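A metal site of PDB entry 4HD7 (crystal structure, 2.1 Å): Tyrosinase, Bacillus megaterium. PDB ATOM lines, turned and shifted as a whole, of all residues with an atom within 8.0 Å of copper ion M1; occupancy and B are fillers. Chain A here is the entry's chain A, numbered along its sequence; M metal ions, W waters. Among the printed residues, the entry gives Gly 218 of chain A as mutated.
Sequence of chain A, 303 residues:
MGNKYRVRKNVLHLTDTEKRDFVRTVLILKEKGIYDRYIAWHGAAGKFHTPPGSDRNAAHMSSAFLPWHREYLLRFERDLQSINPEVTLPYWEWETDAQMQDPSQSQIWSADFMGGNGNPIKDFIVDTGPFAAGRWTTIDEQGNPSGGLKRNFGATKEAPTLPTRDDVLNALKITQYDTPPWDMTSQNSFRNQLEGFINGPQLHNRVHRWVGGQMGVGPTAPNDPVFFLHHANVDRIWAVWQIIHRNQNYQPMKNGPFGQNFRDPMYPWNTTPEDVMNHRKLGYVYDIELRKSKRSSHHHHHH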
ATOM      1  N   HIS A  42     -15.296  28.102   4.212  1.00  0.00           N
ATOM      2  CA  HIS A  42     -14.015  28.737   3.894  1.00  0.00           C
ATOM      3  C   HIS A  42     -14.096  29.661   2.680  1.00  0.00           C
ATOM      4  O   HIS A  42     -13.590  30.790   2.720  1.00  0.00           O
ATOM      5  CB  HIS A  42     -12.938  27.670   3.675  1.00  0.00           C
ATOM      6  CG  HIS A  42     -11.557  28.231   3.624  1.00  0.00           C
ATOM      7  ND1 HIS A  42     -10.981  28.645   2.446  1.00  0.00           N
ATOM      8  CD2 HIS A  42     -10.628  28.435   4.585  1.00  0.00           C
ATOM      9  CE1 HIS A  42      -9.753  29.073   2.680  1.00  0.00           C
ATOM     10  NE2 HIS A  42      -9.509  28.954   3.983  1.00  0.00           N
ATOM     11  N   GLY A  43     -14.712  29.195   1.594  1.00  0.00           N
ATOM     12  CA  GLY A  43     -14.882  30.029   0.408  1.00  0.00           C
ATOM     13  C   GLY A  43     -15.706  31.270   0.693  1.00  0.00           C
ATOM     14  O   GLY A  43     -15.308  32.390   0.369  1.00  0.00           O
ATOM     15  N   ALA A  45     -16.121  32.725   3.446  1.00  0.00           N
ATOM     16  CA  ALA A  45     -15.497  33.635   4.402  1.00  0.00           C
ATOM     17  C   ALA A  45     -14.517  34.546   3.692  1.00  0.00           C
ATOM     18  O   ALA A  45     -14.469  35.742   3.972  1.00  0.00           O
ATOM     19  CB  ALA A  45     -14.797  32.864   5.538  1.00  0.00           C
ATOM     20  N   GLY A  46     -13.768  33.992   2.737  1.00  0.00           N
ATOM     21  CA  GLY A  46     -12.699  34.715   2.079  1.00  0.00           C
ATOM     22  C   GLY A  46     -13.219  35.775   1.145  1.00  0.00           C
ATOM     23  O   GLY A  46     -12.486  36.694   0.782  1.00  0.00           O
ATOM     24  N   ASN A  57     -10.553  40.048   4.907  1.00  0.00           N
ATOM     25  CA  ASN A  57     -11.797  39.292   4.908  1.00  0.00           C
ATOM     26  C   ASN A  57     -11.921  38.594   6.243  1.00  0.00           C
ATOM     27  O   ASN A  57     -11.010  38.656   7.064  1.00  0.00           O
ATOM     28  CB  ASN A  57     -11.901  38.311   3.716  1.00  0.00           C
ATOM     29  CG  ASN A  57     -10.781  37.270   3.670  1.00  0.00           C
ATOM     30  OD1 ASN A  57      -9.845  37.385   2.865  1.00  0.00           O
ATOM     31  ND2 ASN A  57     -10.895  36.237   4.478  1.00  0.00           N
ATOM     32  N   ALA A  59     -11.735  35.596   7.217  1.00  0.00           N
ATOM     33  CA  ALA A  59     -10.898  34.438   7.509  1.00  0.00           C
ATOM     34  C   ALA A  59      -9.404  34.635   7.255  1.00  0.00           C
ATOM     35  O   ALA A  59      -8.617  33.766   7.621  1.00  0.00           O
ATOM     36  CB  ALA A  59     -11.411  33.219   6.746  1.00  0.00           C
ATOM     37  N   HIS A  60      -9.031  35.748   6.644  1.00  0.00           N
ATOM     38  CA  HIS A  60      -7.624  35.969   6.238  1.00  0.00           C
ATOM     39  C   HIS A  60      -7.213  37.436   6.182  1.00  0.00           C
ATOM     40  O   HIS A  60      -8.054  38.336   6.111  1.00  0.00           O
ATOM     41  CB  HIS A  60      -7.353  35.341   4.872  1.00  0.00           C
ATOM     42  CG  HIS A  60      -7.823  33.920   4.749  1.00  0.00           C
ATOM     43  ND1 HIS A  60      -9.053  33.592   4.233  1.00  0.00           N
ATOM     44  CD2 HIS A  60      -7.221  32.746   5.078  1.00  0.00           C
ATOM     45  CE1 HIS A  60      -9.198  32.268   4.250  1.00  0.00           C
ATOM     46  NE2 HIS A  60      -8.097  31.747   4.739  1.00  0.00           N
ATOM     47  N   PHE A  65      -7.833  36.071  11.391  1.00  0.00           N
ATOM     48  CA  PHE A  65      -7.199  34.905  10.792  1.00  0.00           C
ATOM     49  C   PHE A  65      -7.030  33.744  11.766  1.00  0.00           C
ATOM     50  O   PHE A  65      -7.529  32.641  11.505  1.00  0.00           O
ATOM     51  CB  PHE A  65      -5.834  35.289  10.175  1.00  0.00           C
ATOM     52  CG  PHE A  65      -5.034  34.125   9.690  1.00  0.00           C
ATOM     53  CD1 PHE A  65      -5.547  33.240   8.752  1.00  0.00           C
ATOM     54  CD2 PHE A  65      -3.767  33.900  10.175  1.00  0.00           C
ATOM     55  CE1 PHE A  65      -4.795  32.164   8.307  1.00  0.00           C
ATOM     56  CE2 PHE A  65      -3.015  32.828   9.740  1.00  0.00           C
ATOM     57  CZ  PHE A  65      -3.529  31.970   8.791  1.00  0.00           C
ATOM     58  N   TRP A  68     -10.519  32.648  13.604  1.00  0.00           N
ATOM     59  CA  TRP A  68     -11.358  32.040  12.559  1.00  0.00           C
ATOM     60  C   TRP A  68     -11.044  30.556  12.369  1.00  0.00           C
ATOM     61  O   TRP A  68     -11.907  29.689  12.536  1.00  0.00           O
ATOM     62  CB  TRP A  68     -11.221  32.778  11.210  1.00  0.00           C
ATOM     63  CG  TRP A  68     -12.365  32.458  10.258  1.00  0.00           C
ATOM     64  CD1 TRP A  68     -13.521  33.178  10.088  1.00  0.00           C
ATOM     65  CD2 TRP A  68     -12.481  31.327   9.376  1.00  0.00           C
ATOM     66  NE1 TRP A  68     -14.336  32.578   9.148  1.00  0.00           N
ATOM     67  CE2 TRP A  68     -13.722  31.437   8.699  1.00  0.00           C
ATOM     68  CE3 TRP A  68     -11.655  30.239   9.078  1.00  0.00           C
ATOM     69  CZ2 TRP A  68     -14.155  30.502   7.762  1.00  0.00           C
ATOM     70  CZ3 TRP A  68     -12.081  29.307   8.128  1.00  0.00           C
ATOM     71  CH2 TRP A  68     -13.324  29.444   7.485  1.00  0.00           C
ATOM     72  N   HIS A  69      -9.782  30.255  12.051  1.00  0.00           N
ATOM     73  CA  HIS A  69      -9.413  28.886  11.758  1.00  0.00           C
ATOM     74  C   HIS A  69      -9.483  28.002  12.993  1.00  0.00           C
ATOM     75  O   HIS A  69      -9.858  26.839  12.887  1.00  0.00           O
ATOM     76  CB  HIS A  69      -8.033  28.796  11.059  1.00  0.00           C
ATOM     77  CG  HIS A  69      -8.036  29.358   9.672  1.00  0.00           C
ATOM     78  ND1 HIS A  69      -7.847  30.707   9.413  1.00  0.00           N
ATOM     79  CD2 HIS A  69      -8.269  28.792   8.471  1.00  0.00           C
ATOM     80  CE1 HIS A  69      -7.939  30.923   8.115  1.00  0.00           C
ATOM     81  NE2 HIS A  69      -8.176  29.769   7.512  1.00  0.00           N
ATOM     82  N   TYR A  72     -12.939  27.026  13.116  1.00  0.00           N
ATOM     83  CA  TYR A  72     -13.169  26.160  11.939  1.00  0.00           C
ATOM     84  C   TYR A  72     -12.725  24.723  12.260  1.00  0.00           C
ATOM     85  O   TYR A  72     -13.457  23.767  12.008  1.00  0.00           O
ATOM     86  CB  TYR A  72     -12.414  26.737  10.743  1.00  0.00           C
ATOM     87  CG  TYR A  72     -12.545  26.033   9.384  1.00  0.00           C
ATOM     88  CD1 TYR A  72     -13.637  26.277   8.549  1.00  0.00           C
ATOM     89  CD2 TYR A  72     -11.525  25.211   8.892  1.00  0.00           C
ATOM     90  CE1 TYR A  72     -13.733  25.683   7.280  1.00  0.00           C
ATOM     91  CE2 TYR A  72     -11.613  24.603   7.649  1.00  0.00           C
ATOM     92  CZ  TYR A  72     -12.714  24.847   6.835  1.00  0.00           C
ATOM     93  OH  TYR A  72     -12.824  24.246   5.589  1.00  0.00           O
ATOM     94  N   GLU A 195       1.018  34.461   9.577  1.00  0.00           N
ATOM     95  CA  GLU A 195       0.208  34.309   8.378  1.00  0.00           C
ATOM     96  C   GLU A 195       1.126  34.345   7.173  1.00  0.00           C
ATOM     97  O   GLU A 195       0.889  33.698   6.162  1.00  0.00           O
ATOM     98  CB  GLU A 195      -0.867  35.406   8.287  1.00  0.00           C
ATOM     99  CG  GLU A 195      -1.803  35.239   7.098  1.00  0.00           C
ATOM    100  CD  GLU A 195      -3.080  36.103   7.190  1.00  0.00           C
ATOM    101  OE1 GLU A 195      -4.033  35.807   6.409  1.00  0.00           O
ATOM    102  OE2 GLU A 195      -3.133  37.055   8.023  1.00  0.00           O
ATOM    103  N   HIS A 204       2.802  30.368   7.128  1.00  0.00           N
ATOM    104  CA  HIS A 204       1.528  29.839   6.704  1.00  0.00           C
ATOM    105  C   HIS A 204       1.314  29.947   5.184  1.00  0.00           C
ATOM    106  O   HIS A 204       1.122  28.948   4.526  1.00  0.00           O
ATOM    107  CB  HIS A 204       0.364  30.508   7.448  1.00  0.00           C
ATOM    108  CG  HIS A 204      -0.951  30.312   6.805  1.00  0.00           C
ATOM    109  ND1 HIS A 204      -1.488  31.225   5.902  1.00  0.00           N
ATOM    110  CD2 HIS A 204      -1.863  29.309   6.891  1.00  0.00           C
ATOM    111  CE1 HIS A 204      -2.660  30.787   5.493  1.00  0.00           C
ATOM    112  NE2 HIS A 204      -2.910  29.633   6.083  1.00  0.00           N
ATOM    113  N   HIS A 208       1.149  26.885   1.828  1.00  0.00           N
ATOM    114  CA  HIS A 208       0.114  26.742   0.774  1.00  0.00           C
ATOM    115  C   HIS A 208       0.761  26.806  -0.603  1.00  0.00           C
ATOM    116  O   HIS A 208       0.470  25.995  -1.482  1.00  0.00           O
ATOM    117  CB  HIS A 208      -0.959  27.848   0.851  1.00  0.00           C
ATOM    118  CG  HIS A 208      -1.945  27.648   1.963  1.00  0.00           C
ATOM    119  ND1 HIS A 208      -3.005  26.777   1.866  1.00  0.00           N
ATOM    120  CD2 HIS A 208      -2.047  28.247   3.178  1.00  0.00           C
ATOM    121  CE1 HIS A 208      -3.711  26.821   2.987  1.00  0.00           C
ATOM    122  NE2 HIS A 208      -3.150  27.690   3.796  1.00  0.00           N
ATOM    123  N   GLY A 218      -6.536  29.963  -2.131  1.00  0.00           N
ATOM    124  CA  GLY A 218      -7.321  29.971  -0.916  1.00  0.00           C
ATOM    125  C   GLY A 218      -8.671  29.290  -1.011  1.00  0.00           C
ATOM    126  O   GLY A 218      -8.934  28.336  -0.282  1.00  0.00           O
ATOM    127  N   PRO A 219      -9.516  29.766  -1.929  1.00  0.00           N
ATOM    128  CA  PRO A 219     -10.891  29.286  -2.151  1.00  0.00           C
ATOM    129  C   PRO A 219     -11.052  27.766  -2.298  1.00  0.00           C
ATOM    130  O   PRO A 219     -12.143  27.258  -2.081  1.00  0.00           O
ATOM    131  CB  PRO A 219     -11.290  29.959  -3.471  1.00  0.00           C
ATOM    132  CG  PRO A 219     -10.503  31.191  -3.498  1.00  0.00           C
ATOM    133  CD  PRO A 219      -9.163  30.814  -2.901  1.00  0.00           C
ATOM    134  N   ALA A 221      -8.478  25.492  -1.173  1.00  0.00           N
ATOM    135  CA  ALA A 221      -7.557  24.855  -0.246  1.00  0.00           C
ATOM    136  C   ALA A 221      -8.099  23.621   0.497  1.00  0.00           C
ATOM    137  O   ALA A 221      -7.481  22.557   0.446  1.00  0.00           O
ATOM    138  CB  ALA A 221      -6.995  25.906   0.731  1.00  0.00           C
ATOM    139  N   PRO A 222      -9.267  23.745   1.151  1.00  0.00           N
ATOM    140  CA  PRO A 222      -9.783  22.659   1.991  1.00  0.00           C
ATOM    141  C   PRO A 222     -10.245  21.408   1.241  1.00  0.00           C
ATOM    142  O   PRO A 222     -10.546  20.399   1.903  1.00  0.00           O
ATOM    143  CB  PRO A 222     -10.962  23.308   2.762  1.00  0.00           C
ATOM    144  CG  PRO A 222     -10.768  24.808   2.587  1.00  0.00           C
ATOM    145  CD  PRO A 222     -10.097  24.957   1.234  1.00  0.00           C
ATOM    146  N   PHE A 227      -5.159  20.273   4.365  1.00  0.00           N
ATOM    147  CA  PHE A 227      -5.498  21.629   4.803  1.00  0.00           C
ATOM    148  C   PHE A 227      -5.681  21.735   6.300  1.00  0.00           C
ATOM    149  O   PHE A 227      -5.282  22.732   6.915  1.00  0.00           O
ATOM    150  CB  PHE A 227      -6.775  22.115   4.105  1.00  0.00           C
ATOM    151  CG  PHE A 227      -7.248  23.455   4.573  1.00  0.00           C
ATOM    152  CD1 PHE A 227      -8.084  23.578   5.671  1.00  0.00           C
ATOM    153  CD2 PHE A 227      -6.889  24.616   3.891  1.00  0.00           C
ATOM    154  CE1 PHE A 227      -8.538  24.825   6.089  1.00  0.00           C
ATOM    155  CE2 PHE A 227      -7.349  25.864   4.288  1.00  0.00           C
ATOM    156  CZ  PHE A 227      -8.171  25.973   5.390  1.00  0.00           C
ATOM    157  N   HIS A 231      -3.460  23.556   9.176  1.00  0.00           N
ATOM    158  CA  HIS A 231      -4.033  24.508  10.112  1.00  0.00           C
ATOM    159  C   HIS A 231      -3.959  24.069  11.564  1.00  0.00           C
ATOM    160  O   HIS A 231      -3.881  24.906  12.446  1.00  0.00           O
ATOM    161  CB  HIS A 231      -5.418  24.998   9.684  1.00  0.00           C
ATOM    162  CG  HIS A 231      -5.339  26.145   8.716  1.00  0.00           C
ATOM    163  ND1 HIS A 231      -5.271  27.450   9.128  1.00  0.00           N
ATOM    164  CD2 HIS A 231      -5.215  26.145   7.369  1.00  0.00           C
ATOM    165  CE1 HIS A 231      -5.166  28.233   8.048  1.00  0.00           C
ATOM    166  NE2 HIS A 231      -5.120  27.463   6.989  1.00  0.00           N
HETATM  167 CU    CU M   1      -8.281  29.903   5.455  1.00  0.00          CU
HETATM  168 CU    CU M   2      -4.506  28.767   5.319  1.00  0.00          CU
HETATM  169  O   HOH W   1      -6.562  29.258   4.613  1.00  0.00           O
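Copper ion M1 is bound by a ring nitrogen (NE2) of His 60, 2.0 Å away.
Copper ion M1 is bound by water W1.
Copper ion M1 is bound by NE2 of His 69 (2.1 Å).
Copper ion M1 is bound by NE2 of His 42, 2.1 Å away.
The backbone NH (N) of His 60 sits close to the side-chain amide nitrogen (ND2) of Asn 57, 2.9 Å away.
O of Phe 65 lies within hydrogen-bond range of ND1 of His 69, 2.9 Å away.
ND1 of His 42 sits close to O of Gly 218 (3.4 Å).
CZ of Phe 227 touches copper ion M1, 3.9 Å away.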
